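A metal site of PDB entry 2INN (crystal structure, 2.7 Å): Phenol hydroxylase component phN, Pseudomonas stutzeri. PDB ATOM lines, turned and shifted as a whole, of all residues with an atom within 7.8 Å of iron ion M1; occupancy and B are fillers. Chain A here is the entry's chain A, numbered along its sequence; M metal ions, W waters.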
ATOM      1  N   ILE A 104      -1.337  -6.578  13.983  1.00  0.00           N
ATOM      2  CA  ILE A 104      -0.826  -6.449  12.655  1.00  0.00           C
ATOM      3  C   ILE A 104      -1.971  -6.418  11.706  1.00  0.00           C
ATOM      4  O   ILE A 104      -1.991  -5.639  10.751  1.00  0.00           O
ATOM      5  CB  ILE A 104       0.122  -7.567  12.345  1.00  0.00           C
ATOM      6  CG1 ILE A 104       1.563  -7.118  12.540  1.00  0.00           C
ATOM      7  CG2 ILE A 104       0.011  -8.024  10.868  1.00  0.00           C
ATOM      8  CD1 ILE A 104       2.078  -7.147  13.967  1.00  0.00           C
ATOM      9  N   SER A 105      -2.963  -7.250  11.984  1.00  0.00           N
ATOM     10  CA  SER A 105      -4.032  -7.465  11.080  1.00  0.00           C
ATOM     11  C   SER A 105      -4.848  -6.173  10.849  1.00  0.00           C
ATOM     12  O   SER A 105      -5.104  -5.827   9.728  1.00  0.00           O
ATOM     13  CB  SER A 105      -4.829  -8.620  11.627  1.00  0.00           C
ATOM     14  OG  SER A 105      -5.728  -9.076  10.684  1.00  0.00           O
ATOM     15  N   LEU A 107      -3.728  -3.286  10.776  1.00  0.00           N
ATOM     16  CA  LEU A 107      -2.927  -2.506   9.805  1.00  0.00           C
ATOM     17  C   LEU A 107      -3.243  -2.930   8.336  1.00  0.00           C
ATOM     18  O   LEU A 107      -3.290  -2.084   7.402  1.00  0.00           O
ATOM     19  CB  LEU A 107      -1.475  -2.666  10.113  1.00  0.00           C
ATOM     20  CG  LEU A 107      -0.791  -1.756  11.087  1.00  0.00           C
ATOM     21  CD1 LEU A 107      -1.735  -1.165  12.126  1.00  0.00           C
ATOM     22  CD2 LEU A 107       0.318  -2.530  11.750  1.00  0.00           C
ATOM     23  N   GLU A 108      -3.460  -4.218   8.119  1.00  0.00           N
ATOM     24  CA  GLU A 108      -3.869  -4.645   6.826  1.00  0.00           C
ATOM     25  C   GLU A 108      -5.003  -3.723   6.382  1.00  0.00           C
ATOM     26  O   GLU A 108      -4.986  -3.167   5.264  1.00  0.00           O
ATOM     27  CB  GLU A 108      -4.317  -6.148   6.779  1.00  0.00           C
ATOM     28  CG  GLU A 108      -3.149  -7.172   6.926  1.00  0.00           C
ATOM     29  CD  GLU A 108      -1.942  -7.007   5.963  1.00  0.00           C
ATOM     30  OE1 GLU A 108      -0.969  -7.777   6.099  1.00  0.00           O
ATOM     31  OE2 GLU A 108      -1.911  -6.159   5.058  1.00  0.00           O
ATOM     32  N   HIS A 109      -5.980  -3.545   7.262  1.00  0.00           N
ATOM     33  CA  HIS A 109      -7.175  -2.805   6.850  1.00  0.00           C
ATOM     34  C   HIS A 109      -6.892  -1.298   6.763  1.00  0.00           C
ATOM     35  O   HIS A 109      -7.411  -0.576   5.910  1.00  0.00           O
ATOM     36  CB  HIS A 109      -8.293  -3.029   7.849  1.00  0.00           C
ATOM     37  CG  HIS A 109      -9.621  -3.061   7.234  1.00  0.00           C
ATOM     38  ND1 HIS A 109     -10.110  -4.187   6.589  1.00  0.00           N
ATOM     39  CD2 HIS A 109     -10.636  -2.148   7.231  1.00  0.00           C
ATOM     40  CE1 HIS A 109     -11.369  -3.954   6.208  1.00  0.00           C
ATOM     41  NE2 HIS A 109     -11.704  -2.717   6.571  1.00  0.00           N
ATOM     42  N   ALA A 111      -4.263   0.011   5.623  1.00  0.00           N
ATOM     43  CA  ALA A 111      -3.694   0.037   4.276  1.00  0.00           C
ATOM     44  C   ALA A 111      -4.792  -0.024   3.123  1.00  0.00           C
ATOM     45  O   ALA A 111      -4.831   0.842   2.219  1.00  0.00           O
ATOM     46  CB  ALA A 111      -2.635  -1.065   4.149  1.00  0.00           C
ATOM     47  N   PHE A 112      -5.694  -1.013   3.172  1.00  0.00           N
ATOM     48  CA  PHE A 112      -6.804  -1.014   2.237  1.00  0.00           C
ATOM     49  C   PHE A 112      -7.399   0.375   2.132  1.00  0.00           C
ATOM     50  O   PHE A 112      -7.639   0.836   1.051  1.00  0.00           O
ATOM     51  CB  PHE A 112      -7.892  -1.968   2.740  1.00  0.00           C
ATOM     52  CG  PHE A 112      -9.245  -1.681   2.166  1.00  0.00           C
ATOM     53  CD1 PHE A 112      -9.476  -1.785   0.827  1.00  0.00           C
ATOM     54  CD2 PHE A 112     -10.264  -1.291   2.978  1.00  0.00           C
ATOM     55  CE1 PHE A 112     -10.720  -1.536   0.299  1.00  0.00           C
ATOM     56  CE2 PHE A 112     -11.477  -1.016   2.464  1.00  0.00           C
ATOM     57  CZ  PHE A 112     -11.719  -1.141   1.118  1.00  0.00           C
ATOM     58  N   GLN A 134      -3.135  -2.356  -4.950  1.00  0.00           N
ATOM     59  CA  GLN A 134      -2.561  -2.648  -3.674  1.00  0.00           C
ATOM     60  C   GLN A 134      -3.692  -2.573  -2.641  1.00  0.00           C
ATOM     61  O   GLN A 134      -3.998  -3.521  -1.929  1.00  0.00           O
ATOM     62  CB  GLN A 134      -1.399  -1.750  -3.335  1.00  0.00           C
ATOM     63  CG  GLN A 134      -0.983  -2.066  -1.973  1.00  0.00           C
ATOM     64  CD  GLN A 134       0.516  -2.100  -1.761  1.00  0.00           C
ATOM     65  OE1 GLN A 134       1.278  -1.934  -2.709  1.00  0.00           O
ATOM     66  NE2 GLN A 134       0.967  -2.378  -0.497  1.00  0.00           N
ATOM     67  N   ASP A 137      -5.596  -5.682  -2.570  1.00  0.00           N
ATOM     68  CA  ASP A 137      -4.840  -6.743  -2.009  1.00  0.00           C
ATOM     69  C   ASP A 137      -4.901  -6.660  -0.489  1.00  0.00           C
ATOM     70  O   ASP A 137      -4.934  -7.670   0.217  1.00  0.00           O
ATOM     71  CB  ASP A 137      -3.349  -6.608  -2.385  1.00  0.00           C
ATOM     72  CG  ASP A 137      -3.044  -7.035  -3.808  1.00  0.00           C
ATOM     73  OD1 ASP A 137      -3.767  -7.914  -4.350  1.00  0.00           O
ATOM     74  OD2 ASP A 137      -2.065  -6.413  -4.354  1.00  0.00           O
ATOM     75  N   GLU A 138      -4.821  -5.445   0.027  1.00  0.00           N
ATOM     76  CA  GLU A 138      -4.694  -5.284   1.483  1.00  0.00           C
ATOM     77  C   GLU A 138      -6.027  -5.621   2.066  1.00  0.00           C
ATOM     78  O   GLU A 138      -6.086  -6.171   3.157  1.00  0.00           O
ATOM     79  CB  GLU A 138      -4.159  -3.911   1.953  1.00  0.00           C
ATOM     80  CG  GLU A 138      -2.787  -3.524   1.359  1.00  0.00           C
ATOM     81  CD  GLU A 138      -1.631  -4.413   1.794  1.00  0.00           C
ATOM     82  OE1 GLU A 138      -0.437  -4.093   1.473  1.00  0.00           O
ATOM     83  OE2 GLU A 138      -1.895  -5.504   2.372  1.00  0.00           O
ATOM     84  N   LEU A 139      -7.080  -5.418   1.293  1.00  0.00           N
ATOM     85  CA  LEU A 139      -8.388  -5.802   1.789  1.00  0.00           C
ATOM     86  C   LEU A 139      -8.393  -7.325   1.818  1.00  0.00           C
ATOM     87  O   LEU A 139      -8.790  -7.901   2.829  1.00  0.00           O
ATOM     88  CB  LEU A 139      -9.478  -5.310   0.886  1.00  0.00           C
ATOM     89  CG  LEU A 139     -10.868  -5.713   1.282  1.00  0.00           C
ATOM     90  CD1 LEU A 139     -11.420  -4.989   2.545  1.00  0.00           C
ATOM     91  CD2 LEU A 139     -11.780  -5.524   0.110  1.00  0.00           C
ATOM     92  N   ARG A 140      -7.969  -7.994   0.725  1.00  0.00           N
ATOM     93  CA  ARG A 140      -7.761  -9.417   0.821  1.00  0.00           C
ATOM     94  C   ARG A 140      -6.972  -9.891   2.019  1.00  0.00           C
ATOM     95  O   ARG A 140      -7.393 -10.836   2.704  1.00  0.00           O
ATOM     96  CB  ARG A 140      -7.055  -9.915  -0.384  1.00  0.00           C
ATOM     97  CG  ARG A 140      -6.658 -11.358  -0.250  1.00  0.00           C
ATOM     98  CD  ARG A 140      -6.318 -12.109  -1.547  1.00  0.00           C
ATOM     99  NE  ARG A 140      -4.997 -12.686  -1.342  1.00  0.00           N
ATOM    100  CZ  ARG A 140      -4.638 -13.981  -1.536  1.00  0.00           C
ATOM    101  NH1 ARG A 140      -5.504 -14.918  -1.948  1.00  0.00           N
ATOM    102  NH2 ARG A 140      -3.371 -14.328  -1.340  1.00  0.00           N
ATOM    103  N   HIS A 141      -5.797  -9.328   2.241  1.00  0.00           N
ATOM    104  CA  HIS A 141      -5.034  -9.666   3.402  1.00  0.00           C
ATOM    105  C   HIS A 141      -5.956  -9.552   4.606  1.00  0.00           C
ATOM    106  O   HIS A 141      -5.981 -10.458   5.433  1.00  0.00           O
ATOM    107  CB  HIS A 141      -3.825  -8.731   3.572  1.00  0.00           C
ATOM    108  CG  HIS A 141      -2.802  -8.966   2.517  1.00  0.00           C
ATOM    109  ND1 HIS A 141      -1.543  -8.392   2.542  1.00  0.00           N
ATOM    110  CD2 HIS A 141      -2.863  -9.768   1.412  1.00  0.00           C
ATOM    111  CE1 HIS A 141      -0.855  -8.832   1.487  1.00  0.00           C
ATOM    112  NE2 HIS A 141      -1.621  -9.683   0.797  1.00  0.00           N
ATOM    113  N   SER A 142      -6.709  -8.449   4.745  1.00  0.00           N
ATOM    114  CA  SER A 142      -7.451  -8.245   5.990  1.00  0.00           C
ATOM    115  C   SER A 142      -8.546  -9.286   6.190  1.00  0.00           C
ATOM    116  O   SER A 142      -8.612  -9.941   7.213  1.00  0.00           O
ATOM    117  CB  SER A 142      -8.016  -6.842   6.063  1.00  0.00           C
ATOM    118  OG  SER A 142      -8.802  -6.598   7.218  1.00  0.00           O
ATOM    119  N   GLN A 145      -6.960 -12.953   6.885  1.00  0.00           N
ATOM    120  CA  GLN A 145      -6.557 -13.150   8.240  1.00  0.00           C
ATOM    121  C   GLN A 145      -7.734 -13.360   9.184  1.00  0.00           C
ATOM    122  O   GLN A 145      -7.643 -14.077  10.138  1.00  0.00           O
ATOM    123  CB  GLN A 145      -5.755 -11.941   8.650  1.00  0.00           C
ATOM    124  CG  GLN A 145      -4.723 -11.693   7.588  1.00  0.00           C
ATOM    125  CD  GLN A 145      -3.693 -10.682   7.899  1.00  0.00           C
ATOM    126  OE1 GLN A 145      -3.764  -9.984   8.867  1.00  0.00           O
ATOM    127  NE2 GLN A 145      -2.680 -10.632   7.074  1.00  0.00           N
ATOM    128  N   PHE A 198       7.870   0.509   4.728  1.00  0.00           N
ATOM    129  CA  PHE A 198       7.336  -0.664   5.420  1.00  0.00           C
ATOM    130  C   PHE A 198       7.312  -1.818   4.433  1.00  0.00           C
ATOM    131  O   PHE A 198       7.948  -2.826   4.656  1.00  0.00           O
ATOM    132  CB  PHE A 198       5.934  -0.305   5.761  1.00  0.00           C
ATOM    133  CG  PHE A 198       5.188  -1.214   6.728  1.00  0.00           C
ATOM    134  CD1 PHE A 198       5.540  -1.277   8.100  1.00  0.00           C
ATOM    135  CD2 PHE A 198       3.934  -1.798   6.291  1.00  0.00           C
ATOM    136  CE1 PHE A 198       4.703  -1.988   9.033  1.00  0.00           C
ATOM    137  CE2 PHE A 198       3.094  -2.543   7.165  1.00  0.00           C
ATOM    138  CZ  PHE A 198       3.460  -2.639   8.527  1.00  0.00           C
ATOM    139  N   GLU A 199       6.613  -1.639   3.319  1.00  0.00           N
ATOM    140  CA  GLU A 199       6.499  -2.699   2.379  1.00  0.00           C
ATOM    141  C   GLU A 199       7.824  -3.058   1.679  1.00  0.00           C
ATOM    142  O   GLU A 199       8.011  -4.182   1.238  1.00  0.00           O
ATOM    143  CB  GLU A 199       5.194  -2.634   1.516  1.00  0.00           C
ATOM    144  CG  GLU A 199       3.823  -2.714   2.345  1.00  0.00           C
ATOM    145  CD  GLU A 199       2.765  -3.777   1.882  1.00  0.00           C
ATOM    146  OE1 GLU A 199       1.619  -3.837   2.375  1.00  0.00           O
ATOM    147  OE2 GLU A 199       3.038  -4.606   1.033  1.00  0.00           O
ATOM    148  N   THR A 203       9.576  -4.983   5.245  1.00  0.00           N
ATOM    149  CA  THR A 203       8.566  -5.975   5.092  1.00  0.00           C
ATOM    150  C   THR A 203       8.995  -7.429   5.542  1.00  0.00           C
ATOM    151  O   THR A 203       8.201  -8.170   6.163  1.00  0.00           O
ATOM    152  CB  THR A 203       8.086  -5.995   3.637  1.00  0.00           C
ATOM    153  OG1 THR A 203       6.882  -6.742   3.506  1.00  0.00           O
ATOM    154  CG2 THR A 203       9.093  -6.693   2.770  1.00  0.00           C
ATOM    155  N   PHE A 207       7.273 -10.095   8.259  1.00  0.00           N
ATOM    156  CA  PHE A 207       6.517 -11.092   7.538  1.00  0.00           C
ATOM    157  C   PHE A 207       7.175 -12.407   7.802  1.00  0.00           C
ATOM    158  O   PHE A 207       6.554 -13.272   8.389  1.00  0.00           O
ATOM    159  CB  PHE A 207       6.520 -10.769   6.037  1.00  0.00           C
ATOM    160  CG  PHE A 207       5.565 -11.626   5.193  1.00  0.00           C
ATOM    161  CD1 PHE A 207       6.082 -12.716   4.388  1.00  0.00           C
ATOM    162  CD2 PHE A 207       4.147 -11.337   5.176  1.00  0.00           C
ATOM    163  CE1 PHE A 207       5.202 -13.521   3.552  1.00  0.00           C
ATOM    164  CE2 PHE A 207       3.251 -12.149   4.362  1.00  0.00           C
ATOM    165  CZ  PHE A 207       3.806 -13.253   3.534  1.00  0.00           C
ATOM    166  N   PHE A 225      -1.674 -18.873   4.684  1.00  0.00           N
ATOM    167  CA  PHE A 225      -2.127 -17.589   4.304  1.00  0.00           C
ATOM    168  C   PHE A 225      -0.818 -16.966   3.679  1.00  0.00           C
ATOM    169  O   PHE A 225      -0.871 -16.305   2.546  1.00  0.00           O
ATOM    170  CB  PHE A 225      -2.679 -16.786   5.476  1.00  0.00           C
ATOM    171  CG  PHE A 225      -2.414 -15.347   5.291  1.00  0.00           C
ATOM    172  CD1 PHE A 225      -3.153 -14.577   4.270  1.00  0.00           C
ATOM    173  CD2 PHE A 225      -1.308 -14.706   5.965  1.00  0.00           C
ATOM    174  CE1 PHE A 225      -2.908 -13.169   4.015  1.00  0.00           C
ATOM    175  CE2 PHE A 225      -0.995 -13.250   5.729  1.00  0.00           C
ATOM    176  CZ  PHE A 225      -1.811 -12.471   4.791  1.00  0.00           C
ATOM    177  N   ALA A 229       0.071 -15.238   0.187  1.00  0.00           N
ATOM    178  CA  ALA A 229       0.406 -13.785   0.137  1.00  0.00           C
ATOM    179  C   ALA A 229       1.742 -13.431  -0.574  1.00  0.00           C
ATOM    180  O   ALA A 229       1.993 -12.267  -0.877  1.00  0.00           O
ATOM    181  CB  ALA A 229       0.464 -13.151   1.535  1.00  0.00           C
ATOM    182  N   ASP A 232       1.386 -11.607  -3.862  1.00  0.00           N
ATOM    183  CA  ASP A 232       0.932 -10.271  -3.497  1.00  0.00           C
ATOM    184  C   ASP A 232       2.091  -9.384  -3.100  1.00  0.00           C
ATOM    185  O   ASP A 232       2.315  -8.434  -3.780  1.00  0.00           O
ATOM    186  CB  ASP A 232      -0.024 -10.351  -2.344  1.00  0.00           C
ATOM    187  CG  ASP A 232      -1.342 -10.954  -2.726  1.00  0.00           C
ATOM    188  OD1 ASP A 232      -1.650 -11.059  -3.950  1.00  0.00           O
ATOM    189  OD2 ASP A 232      -2.085 -11.276  -1.770  1.00  0.00           O
ATOM    190  N   GLU A 233       2.860  -9.703  -2.054  1.00  0.00           N
ATOM    191  CA  GLU A 233       3.995  -8.902  -1.640  1.00  0.00           C
ATOM    192  C   GLU A 233       4.995  -8.617  -2.810  1.00  0.00           C
ATOM    193  O   GLU A 233       5.532  -7.520  -2.923  1.00  0.00           O
ATOM    194  CB  GLU A 233       4.677  -9.555  -0.450  1.00  0.00           C
ATOM    195  CG  GLU A 233       3.780  -9.849   0.836  1.00  0.00           C
ATOM    196  CD  GLU A 233       3.010  -8.591   1.588  1.00  0.00           C
ATOM    197  OE1 GLU A 233       2.627  -8.784   2.779  1.00  0.00           O
ATOM    198  OE2 GLU A 233       2.774  -7.451   1.029  1.00  0.00           O
ATOM    199  N   HIS A 236       3.785  -5.735  -4.115  1.00  0.00           N
ATOM    200  CA  HIS A 236       3.819  -4.557  -3.283  1.00  0.00           C
ATOM    201  C   HIS A 236       5.227  -4.018  -3.217  1.00  0.00           C
ATOM    202  O   HIS A 236       5.381  -2.823  -3.292  1.00  0.00           O
ATOM    203  CB  HIS A 236       3.197  -4.769  -1.935  1.00  0.00           C
ATOM    204  CG  HIS A 236       1.801  -5.287  -1.995  1.00  0.00           C
ATOM    205  ND1 HIS A 236       1.077  -5.648  -0.858  1.00  0.00           N
ATOM    206  CD2 HIS A 236       0.982  -5.558  -3.053  1.00  0.00           C
ATOM    207  CE1 HIS A 236      -0.121  -6.092  -1.237  1.00  0.00           C
ATOM    208  NE2 HIS A 236      -0.199  -6.042  -2.552  1.00  0.00           N
HETATM  209 FE    FE M   1      -0.653  -6.742   3.491  1.00  0.00          FE
HETATM  210 FE    FE M   2       1.428  -5.905   1.311  1.00  0.00          FE
HETATM  211  O   HOH W   1       0.904  -8.278   4.664  1.00  0.00           O
HETATM  212  O   HOH W   2       0.080  -5.248   4.348  1.00  0.00           O
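The side-chain carboxylate of Glu 108 sits at hydrogen-bond distance from the side-chain amide nitrogen of Gln 145. NE2 of Gln 134 lies within hydrogen-bond range of OE1 of Glu 138, at 3.0 Å. The side-chain amide nitrogen (NE2) of Gln 134 lies close to the side-chain carboxylate (OE1) of Glu 199, 3.3 Å away. The side-chain carboxylate (OE1) of Glu 138 sits close to a ring nitrogen (ND1) of His 236 (3.2 Å). NE2 of His 141 lies within hydrogen-bond range of OD2 of Asp 232, 3.1 Å away.
Residues that only touch iron ion M1: Glu 199 (3.9 Å) and Glu 233 (3.9 Å). Of the 24 residues printed, 5 come within 4 Å of iron ion M1. The nearest printed residue that does not touch iron ion M1 is His 236 (4.8 Å).
Iron ion M1 is bound by water W2 (1.9 Å), the side-chain carboxylate (OE2) of Glu 138 (2.1 Å), the side-chain carboxylate (OE2) of Glu 108 (2.1 Å), a ring nitrogen (ND1) of His 141 (2.1 Å) and water W1 (2.5 Å). Iron ion M1 has five donor atoms within binding distance. Slightly farther from iron ion M1 lies the side-chain carboxylate (OE1) of Glu 108 (2.8 Å).
Water W1 lies within hydrogen-bond range of OE1 of Glu 108 (2.4 Å) and OE1 of Glu 233 (2.6 Å). Water W2 bridges OE1 of Glu 138 (3.1 Å) and OE1 of Glu 108 (3.2 Å).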
